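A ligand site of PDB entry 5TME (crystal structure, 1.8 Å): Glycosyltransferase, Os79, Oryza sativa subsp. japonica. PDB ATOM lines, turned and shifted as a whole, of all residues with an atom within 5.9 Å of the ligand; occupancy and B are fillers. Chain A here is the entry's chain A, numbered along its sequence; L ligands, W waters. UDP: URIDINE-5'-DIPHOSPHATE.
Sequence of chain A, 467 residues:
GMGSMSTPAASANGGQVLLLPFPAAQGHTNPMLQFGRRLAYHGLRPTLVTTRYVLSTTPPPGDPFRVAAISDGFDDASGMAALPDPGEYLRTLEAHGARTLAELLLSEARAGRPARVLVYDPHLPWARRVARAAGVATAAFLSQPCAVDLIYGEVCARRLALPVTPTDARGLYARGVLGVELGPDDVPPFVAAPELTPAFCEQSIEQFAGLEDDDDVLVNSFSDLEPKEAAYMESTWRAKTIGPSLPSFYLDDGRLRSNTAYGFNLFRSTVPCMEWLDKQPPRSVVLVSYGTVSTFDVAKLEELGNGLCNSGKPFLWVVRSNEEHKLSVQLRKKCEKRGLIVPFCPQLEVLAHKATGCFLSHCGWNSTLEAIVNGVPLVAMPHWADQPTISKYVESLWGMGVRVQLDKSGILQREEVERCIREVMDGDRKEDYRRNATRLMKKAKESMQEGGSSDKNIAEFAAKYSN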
ATOM      1  N   ASN A  30      -9.915  34.040  -9.778  1.00  0.00           N
ATOM      2  CA  ASN A  30     -10.510  35.224 -10.303  1.00  0.00           C
ATOM      3  C   ASN A  30     -10.277  36.477  -9.455  1.00  0.00           C
ATOM      4  O   ASN A  30     -10.031  37.513 -10.055  1.00  0.00           O
ATOM      5  CB  ASN A  30     -12.007  35.047 -10.549  1.00  0.00           C
ATOM      6  CG  ASN A  30     -12.309  34.030 -11.615  1.00  0.00           C
ATOM      7  OD1 ASN A  30     -11.952  34.194 -12.787  1.00  0.00           O
ATOM      8  ND2 ASN A  30     -13.025  32.983 -11.222  1.00  0.00           N
ATOM      9  N   SER A 289     -25.633  26.096  -5.230  1.00  0.00           N
ATOM     10  CA  SER A 289     -24.246  25.637  -5.404  1.00  0.00           C
ATOM     11  C   SER A 289     -23.573  25.368  -4.073  1.00  0.00           C
ATOM     12  O   SER A 289     -23.767  26.118  -3.145  1.00  0.00           O
ATOM     13  CB  SER A 289     -23.381  26.661  -6.098  1.00  0.00           C
ATOM     14  OG  SER A 289     -22.084  26.048  -6.358  1.00  0.00           O
ATOM     15  N   TYR A 290     -22.796  24.284  -3.989  1.00  0.00           N
ATOM     16  CA  TYR A 290     -21.947  24.100  -2.799  1.00  0.00           C
ATOM     17  C   TYR A 290     -20.500  24.228  -3.152  1.00  0.00           C
ATOM     18  O   TYR A 290     -19.616  23.838  -2.375  1.00  0.00           O
ATOM     19  CB  TYR A 290     -22.213  22.813  -2.050  1.00  0.00           C
ATOM     20  CG  TYR A 290     -22.142  21.546  -2.850  1.00  0.00           C
ATOM     21  CD1 TYR A 290     -20.920  20.905  -3.100  1.00  0.00           C
ATOM     22  CD2 TYR A 290     -23.304  20.961  -3.324  1.00  0.00           C
ATOM     23  CE1 TYR A 290     -20.898  19.740  -3.844  1.00  0.00           C
ATOM     24  CE2 TYR A 290     -23.310  19.802  -4.071  1.00  0.00           C
ATOM     25  CZ  TYR A 290     -22.101  19.178  -4.371  1.00  0.00           C
ATOM     26  OH  TYR A 290     -22.156  17.980  -5.134  1.00  0.00           O
ATOM     27  N   GLY A 291     -20.253  24.799  -4.312  1.00  0.00           N
ATOM     28  CA  GLY A 291     -18.949  25.224  -4.656  1.00  0.00           C
ATOM     29  C   GLY A 291     -18.128  24.197  -5.419  1.00  0.00           C
ATOM     30  O   GLY A 291     -18.622  23.115  -5.756  1.00  0.00           O
ATOM     31  N   THR A 292     -16.840  24.525  -5.633  1.00  0.00           N
ATOM     32  CA  THR A 292     -16.005  23.806  -6.575  1.00  0.00           C
ATOM     33  C   THR A 292     -15.125  22.789  -5.905  1.00  0.00           C
ATOM     34  O   THR A 292     -14.550  21.934  -6.606  1.00  0.00           O
ATOM     35  CB  THR A 292     -15.112  24.755  -7.402  1.00  0.00           C
ATOM     36  OG1 THR A 292     -14.213  25.432  -6.504  1.00  0.00           O
ATOM     37  CG2 THR A 292     -15.972  25.772  -8.142  1.00  0.00           C
ATOM     38  N   VAL A 293     -15.061  22.838  -4.573  1.00  0.00           N
ATOM     39  CA  VAL A 293     -14.134  22.047  -3.743  1.00  0.00           C
ATOM     40  C   VAL A 293     -14.842  20.995  -2.891  1.00  0.00           C
ATOM     41  O   VAL A 293     -14.459  19.826  -2.920  1.00  0.00           O
ATOM     42  CB  VAL A 293     -13.325  22.964  -2.758  1.00  0.00           C
ATOM     43  CG1 VAL A 293     -12.460  22.149  -1.787  1.00  0.00           C
ATOM     44  CG2 VAL A 293     -12.517  23.985  -3.508  1.00  0.00           C
ATOM     45  N   SER A 294     -15.881  21.351  -2.136  1.00  0.00           N
ATOM     46  CA  SER A 294     -16.516  20.396  -1.221  1.00  0.00           C
ATOM     47  C   SER A 294     -17.106  19.268  -2.026  1.00  0.00           C
ATOM     48  O   SER A 294     -17.569  19.492  -3.151  1.00  0.00           O
ATOM     49  CB  SER A 294     -17.642  21.011  -0.368  1.00  0.00           C
ATOM     50  OG  SER A 294     -17.169  22.047   0.491  1.00  0.00           O
ATOM     51  N   VAL A 318     -26.301  23.631  -9.710  1.00  0.00           N
ATOM     52  CA  VAL A 318     -25.117  23.329 -10.400  1.00  0.00           C
ATOM     53  C   VAL A 318     -24.514  22.147  -9.659  1.00  0.00           C
ATOM     54  O   VAL A 318     -24.193  22.226  -8.495  1.00  0.00           O
ATOM     55  CB  VAL A 318     -24.084  24.500 -10.312  1.00  0.00           C
ATOM     56  CG1 VAL A 318     -22.798  24.079 -11.011  1.00  0.00           C
ATOM     57  CG2 VAL A 318     -24.664  25.724 -10.974  1.00  0.00           C
ATOM     58  N   PRO A 343     -23.854  21.208 -15.160  1.00  0.00           N
ATOM     59  CA  PRO A 343     -22.564  21.025 -14.520  1.00  0.00           C
ATOM     60  C   PRO A 343     -21.811  22.308 -14.259  1.00  0.00           C
ATOM     61  O   PRO A 343     -20.847  22.264 -13.506  1.00  0.00           O
ATOM     62  CB  PRO A 343     -21.775  20.196 -15.551  1.00  0.00           C
ATOM     63  CG  PRO A 343     -22.402  20.542 -16.869  1.00  0.00           C
ATOM     64  CD  PRO A 343     -23.853  20.756 -16.564  1.00  0.00           C
ATOM     65  N   PHE A 344     -22.251  23.414 -14.860  1.00  0.00           N
ATOM     66  CA  PHE A 344     -21.511  24.728 -14.791  1.00  0.00           C
ATOM     67  C   PHE A 344     -22.468  25.803 -15.206  1.00  0.00           C
ATOM     68  O   PHE A 344     -23.217  25.600 -16.155  1.00  0.00           O
ATOM     69  CB  PHE A 344     -20.333  24.810 -15.818  1.00  0.00           C
ATOM     70  CG  PHE A 344     -19.829  26.246 -16.028  1.00  0.00           C
ATOM     71  CD1 PHE A 344     -19.035  26.865 -15.049  1.00  0.00           C
ATOM     72  CD2 PHE A 344     -20.210  27.011 -17.155  1.00  0.00           C
ATOM     73  CE1 PHE A 344     -18.633  28.208 -15.188  1.00  0.00           C
ATOM     74  CE2 PHE A 344     -19.789  28.356 -17.306  1.00  0.00           C
ATOM     75  CZ  PHE A 344     -19.000  28.941 -16.317  1.00  0.00           C
ATOM     76  N   CYS A 345     -22.448  26.940 -14.510  1.00  0.00           N
ATOM     77  CA  CYS A 345     -23.249  28.116 -14.824  1.00  0.00           C
ATOM     78  C   CYS A 345     -22.312  29.288 -14.626  1.00  0.00           C
ATOM     79  O   CYS A 345     -21.517  29.224 -13.723  1.00  0.00           O
ATOM     80  CB  CYS A 345     -24.431  28.255 -13.837  1.00  0.00           C
ATOM     81  SG  CYS A 345     -24.076  29.048 -12.231  1.00  0.00           S
ATOM     82  N   PRO A 346     -22.394  30.354 -15.411  1.00  0.00           N
ATOM     83  CA  PRO A 346     -21.573  31.498 -15.065  1.00  0.00           C
ATOM     84  C   PRO A 346     -22.264  32.214 -13.870  1.00  0.00           C
ATOM     85  O   PRO A 346     -23.273  32.859 -14.017  1.00  0.00           O
ATOM     86  CB  PRO A 346     -21.552  32.311 -16.354  1.00  0.00           C
ATOM     87  CG  PRO A 346     -22.828  31.933 -17.005  1.00  0.00           C
ATOM     88  CD  PRO A 346     -23.120  30.541 -16.701  1.00  0.00           C
ATOM     89  N   GLN A 347     -21.705  32.004 -12.682  1.00  0.00           N
ATOM     90  CA  GLN A 347     -22.429  32.301 -11.473  1.00  0.00           C
ATOM     91  C   GLN A 347     -22.696  33.793 -11.330  1.00  0.00           C
ATOM     92  O   GLN A 347     -23.750  34.150 -10.920  1.00  0.00           O
ATOM     93  CB  GLN A 347     -21.677  31.655 -10.346  1.00  0.00           C
ATOM     94  CG  GLN A 347     -22.077  32.087  -8.998  1.00  0.00           C
ATOM     95  CD  GLN A 347     -21.501  31.205  -7.876  1.00  0.00           C
ATOM     96  OE1 GLN A 347     -21.665  29.961  -7.834  1.00  0.00           O
ATOM     97  NE2 GLN A 347     -20.860  31.842  -6.941  1.00  0.00           N
ATOM     98  N   LEU A 348     -21.738  34.658 -11.651  1.00  0.00           N
ATOM     99  CA  LEU A 348     -21.968  36.085 -11.532  1.00  0.00           C
ATOM    100  C   LEU A 348     -23.075  36.532 -12.472  1.00  0.00           C
ATOM    101  O   LEU A 348     -23.897  37.266 -12.107  1.00  0.00           O
ATOM    102  CB  LEU A 348     -20.750  36.953 -11.887  1.00  0.00           C
ATOM    103  CG  LEU A 348     -19.904  37.320 -10.729  1.00  0.00           C
ATOM    104  CD1 LEU A 348     -18.645  37.850 -11.374  1.00  0.00           C
ATOM    105  CD2 LEU A 348     -20.587  38.350  -9.856  1.00  0.00           C
ATOM    106  N   SER A 361     -26.266  28.488  -0.989  1.00  0.00           N
ATOM    107  CA  SER A 361     -24.879  28.488  -1.213  1.00  0.00           C
ATOM    108  C   SER A 361     -24.163  27.940   0.014  1.00  0.00           C
ATOM    109  O   SER A 361     -24.629  28.118   1.089  1.00  0.00           O
ATOM    110  CB  SER A 361     -24.411  29.923  -1.370  1.00  0.00           C
ATOM    111  OG  SER A 361     -22.989  30.041  -1.519  1.00  0.00           O
ATOM    112  N   HIS A 362     -23.061  27.295  -0.208  1.00  0.00           N
ATOM    113  CA  HIS A 362     -22.170  26.931   0.923  1.00  0.00           C
ATOM    114  C   HIS A 362     -21.513  28.160   1.603  1.00  0.00           C
ATOM    115  O   HIS A 362     -20.927  28.037   2.676  1.00  0.00           O
ATOM    116  CB  HIS A 362     -21.115  25.972   0.445  1.00  0.00           C
ATOM    117  CG  HIS A 362     -20.081  26.563  -0.441  1.00  0.00           C
ATOM    118  ND1 HIS A 362     -20.328  27.271  -1.631  1.00  0.00           N
ATOM    119  CD2 HIS A 362     -18.741  26.515  -0.318  1.00  0.00           C
ATOM    120  CE1 HIS A 362     -19.183  27.668  -2.139  1.00  0.00           C
ATOM    121  NE2 HIS A 362     -18.191  27.151  -1.407  1.00  0.00           N
ATOM    122  N   CYS A 363     -21.627  29.322   0.982  1.00  0.00           N
ATOM    123  CA  CYS A 363     -21.108  30.573   1.541  1.00  0.00           C
ATOM    124  C   CYS A 363     -19.595  30.554   1.710  1.00  0.00           C
ATOM    125  O   CYS A 363     -19.097  31.056   2.691  1.00  0.00           O
ATOM    126  CB  CYS A 363     -21.812  31.002   2.803  1.00  0.00           C
ATOM    127  SG  CYS A 363     -23.456  31.745   2.457  1.00  0.00           S
ATOM    128  N   GLY A 364     -18.931  30.001   0.745  1.00  0.00           N
ATOM    129  CA  GLY A 364     -17.515  30.324   0.396  1.00  0.00           C
ATOM    130  C   GLY A 364     -17.450  31.852   0.159  1.00  0.00           C
ATOM    131  O   GLY A 364     -18.484  32.516  -0.082  1.00  0.00           O
ATOM    132  N   TRP A 365     -16.288  32.445   0.391  1.00  0.00           N
ATOM    133  CA  TRP A 365     -16.208  33.901   0.305  1.00  0.00           C
ATOM    134  C   TRP A 365     -16.498  34.413  -1.097  1.00  0.00           C
ATOM    135  O   TRP A 365     -17.136  35.466  -1.205  1.00  0.00           O
ATOM    136  CB  TRP A 365     -14.827  34.372   0.814  1.00  0.00           C
ATOM    137  CG  TRP A 365     -14.771  35.834   1.091  1.00  0.00           C
ATOM    138  CD1 TRP A 365     -13.743  36.649   0.745  1.00  0.00           C
ATOM    139  CD2 TRP A 365     -15.641  36.633   1.902  1.00  0.00           C
ATOM    140  NE1 TRP A 365     -13.966  37.860   1.248  1.00  0.00           N
ATOM    141  CE2 TRP A 365     -15.100  37.931   1.939  1.00  0.00           C
ATOM    142  CE3 TRP A 365     -16.832  36.417   2.541  1.00  0.00           C
ATOM    143  CZ2 TRP A 365     -15.709  38.970   2.586  1.00  0.00           C
ATOM    144  CZ3 TRP A 365     -17.425  37.443   3.209  1.00  0.00           C
ATOM    145  CH2 TRP A 365     -16.829  38.721   3.236  1.00  0.00           C
ATOM    146  N   ASN A 366     -15.915  33.791  -2.130  1.00  0.00           N
ATOM    147  CA  ASN A 366     -16.219  34.378  -3.504  1.00  0.00           C
ATOM    148  C   ASN A 366     -17.717  34.346  -3.770  1.00  0.00           C
ATOM    149  O   ASN A 366     -18.320  35.346  -4.223  1.00  0.00           O
ATOM    150  CB  ASN A 366     -15.478  33.621  -4.512  1.00  0.00           C
ATOM    151  CG  ASN A 366     -14.026  33.789  -4.322  1.00  0.00           C
ATOM    152  OD1 ASN A 366     -13.542  34.890  -4.379  1.00  0.00           O
ATOM    153  ND2 ASN A 366     -13.331  32.734  -4.065  1.00  0.00           N
ATOM    154  N   SER A 367     -18.367  33.225  -3.442  1.00  0.00           N
ATOM    155  CA  SER A 367     -19.844  33.140  -3.618  1.00  0.00           C
ATOM    156  C   SER A 367     -20.605  34.182  -2.874  1.00  0.00           C
ATOM    157  O   SER A 367     -21.563  34.731  -3.377  1.00  0.00           O
ATOM    158  CB  SER A 367     -20.442  31.750  -3.285  1.00  0.00           C
ATOM    159  OG  SER A 367     -19.906  30.838  -4.255  1.00  0.00           O
ATOM    160  N   THR A 368     -20.197  34.463  -1.620  1.00  0.00           N
ATOM    161  CA  THR A 368     -20.840  35.389  -0.825  1.00  0.00           C
ATOM    162  C   THR A 368     -20.680  36.832  -1.361  1.00  0.00           C
ATOM    163  O   THR A 368     -21.642  37.575  -1.427  1.00  0.00           O
ATOM    164  CB  THR A 368     -20.330  35.298   0.650  1.00  0.00           C
ATOM    165  OG1 THR A 368     -20.543  33.935   1.053  1.00  0.00           O
ATOM    166  CG2 THR A 368     -21.015  36.262   1.566  1.00  0.00           C
ATOM    167  N   GLU A 370     -20.072  37.611  -4.398  1.00  0.00           N
ATOM    168  CA  GLU A 370     -20.835  37.720  -5.722  1.00  0.00           C
ATOM    169  C   GLU A 370     -22.319  37.891  -5.461  1.00  0.00           C
ATOM    170  O   GLU A 370     -22.993  38.604  -6.177  1.00  0.00           O
ATOM    171  CB  GLU A 370     -20.569  36.472  -6.553  1.00  0.00           C
ATOM    172  CG  GLU A 370     -19.113  36.446  -6.994  1.00  0.00           C
ATOM    173  CD  GLU A 370     -18.649  35.174  -7.569  1.00  0.00           C
ATOM    174  OE1 GLU A 370     -19.439  34.257  -7.772  1.00  0.00           O
ATOM    175  OE2 GLU A 370     -17.406  35.112  -7.824  1.00  0.00           O
ATOM    176  N   GLN A 387     -16.653  29.169   5.955  1.00  0.00           N
ATOM    177  CA  GLN A 387     -18.115  29.167   5.669  1.00  0.00           C
ATOM    178  C   GLN A 387     -18.982  29.257   6.866  1.00  0.00           C
ATOM    179  O   GLN A 387     -19.933  30.024   6.891  1.00  0.00           O
ATOM    180  CB  GLN A 387     -18.421  27.968   4.768  1.00  0.00           C
ATOM    181  CG  GLN A 387     -17.582  27.879   3.467  1.00  0.00           C
ATOM    182  CD  GLN A 387     -17.326  26.466   2.995  1.00  0.00           C
ATOM    183  OE1 GLN A 387     -18.013  25.494   3.400  1.00  0.00           O
ATOM    184  NE2 GLN A 387     -16.313  26.331   2.146  1.00  0.00           N
HETATM  185  N1  UDP L   1     -18.198  29.446 -10.206  1.00  0.00           N
HETATM  186  C2  UDP L   1     -18.881  29.680 -11.442  1.00  0.00           C
HETATM  187  N3  UDP L   1     -19.706  28.712 -11.898  1.00  0.00           N
HETATM  188  C4  UDP L   1     -19.960  27.591 -11.194  1.00  0.00           C
HETATM  189  C5  UDP L   1     -19.320  27.352  -9.985  1.00  0.00           C
HETATM  190  C6  UDP L   1     -18.462  28.308  -9.505  1.00  0.00           C
HETATM  191  O2  UDP L   1     -18.748  30.741 -12.124  1.00  0.00           O
HETATM  192  O4  UDP L   1     -20.708  26.716 -11.702  1.00  0.00           O
HETATM  193  C1' UDP L   1     -17.228  30.367  -9.580  1.00  0.00           C
HETATM  194  C2' UDP L   1     -17.898  31.281  -8.568  1.00  0.00           C
HETATM  195  O2' UDP L   1     -18.491  32.404  -9.214  1.00  0.00           O
HETATM  196  C3' UDP L   1     -16.756  31.627  -7.622  1.00  0.00           C
HETATM  197  C4' UDP L   1     -16.015  30.234  -7.411  1.00  0.00           C
HETATM  198  O4' UDP L   1     -16.165  29.684  -8.823  1.00  0.00           O
HETATM  199  O3' UDP L   1     -16.002  32.649  -8.264  1.00  0.00           O
HETATM  200  C5' UDP L   1     -16.540  29.421  -6.145  1.00  0.00           C
HETATM  201  O5' UDP L   1     -15.880  29.892  -4.819  1.00  0.00           O
HETATM  202  PA  UDP L   1     -16.232  30.066  -3.250  1.00  0.00           P
HETATM  203  O1A UDP L   1     -15.164  30.967  -2.515  1.00  0.00           O
HETATM  204  O2A UDP L   1     -17.561  30.604  -2.931  1.00  0.00           O
HETATM  205  O3A UDP L   1     -16.049  28.468  -2.670  1.00  0.00           O
HETATM  206  PB  UDP L   1     -15.098  27.219  -3.292  1.00  0.00           P
HETATM  207  O1B UDP L   1     -15.420  26.265  -2.176  1.00  0.00           O
HETATM  208  O2B UDP L   1     -15.597  26.909  -4.733  1.00  0.00           O
HETATM  209  O3B UDP L   1     -13.654  27.761  -3.184  1.00  0.00           O
HETATM  210  O   HOH W   1     -13.802  26.298  -0.113  1.00  0.00           O
HETATM  211  O   HOH W   2     -18.890  33.691 -11.782  1.00  0.00           O
HETATM  212  O   HOH W   3     -16.790  24.006  -2.304  1.00  0.00           O
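Water W1 bridges O1B of the ligand (2.6 Å) and NE2 of Gln 387 (3.4 Å).
Water W2 lies within hydrogen-bond range of an oxygen (O2') of the ligand (2.9 Å), the backbone NH of Leu 348 (3.0 Å) and the backbone NH of Gln 347 (3.4 Å).
NE2 of Gln 347 is in hydrogen-bond range of OE1 of Glu 370, at 2.9 Å.
The side-chain hydroxyl (OG) of Ser 367 lies within hydrogen-bond range of the side-chain amide nitrogen (NE2) of Gln 347, 3.0 Å away.
The backbone carbonyl oxygen of Ser 289 is in hydrogen-bond range of the backbone NH of His 362.
The side-chain hydroxyl (OG1) of Thr 368 sits at hydrogen-bond distance from the backbone carbonyl oxygen (O) of Gly 364 (2.7 Å).
The backbone NH (N) of Gly 291 is in hydrogen-bond range of the side-chain hydroxyl (OG) of Ser 289 (3.0 Å).
The side-chain carboxylate (OE1) of Glu 370 is in hydrogen-bond range of an oxygen (O2') of the ligand (2.5 Å).
N of Cys 345 is in hydrogen-bond range of O4 of the ligand (3.3 Å).
A nitrogen (N3) of the ligand lies within hydrogen-bond range of the backbone carbonyl oxygen (O) of Cys 345.
The backbone NH of Thr 292 sits at hydrogen-bond distance from an oxygen (O2B) of the ligand.
OG1 of Thr 292 sits at hydrogen-bond distance from O2B of the ligand.
The backbone NH (N) of Ser 367 is in hydrogen-bond range of an oxygen (O2A) of the ligand (2.8 Å).
An oxygen (O2A) of the ligand is in hydrogen-bond range of the side-chain hydroxyl (OG) of Ser 367 (2.7 Å).
A ring nitrogen (NE2) of His 362 lies within hydrogen-bond range of an oxygen (O3A) of the ligand, at 2.8 Å.
N of Asn 366 lies within hydrogen-bond range of O1A of the ligand (2.9 Å).
ND2 of Asn 366 is in hydrogen-bond range of O1A of the ligand (3.0 Å).
An oxygen (O2) of the ligand lies within hydrogen-bond range of the backbone NH of Gln 347.
The side-chain amide nitrogen (NE2) of Gln 347 lies within hydrogen-bond range of an oxygen (O2') of the ligand.
The backbone NH (N) of Trp 365 sits at hydrogen-bond distance from an oxygen (O1A) of the ligand.
Merely in contact with the ligand: Gly 364 (3.3 Å), Val 318 (3.4 Å), Phe 344 (3.5 Å), Gly 291 (3.8 Å) and Val 293 (3.9 Å).
Hydrophobic or aromatic side chains that line the ligand: Val 293, Val 318, Phe 344 and His 362.
The nearest printed residue that does not touch the ligand is Pro 346 (4.1 Å).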
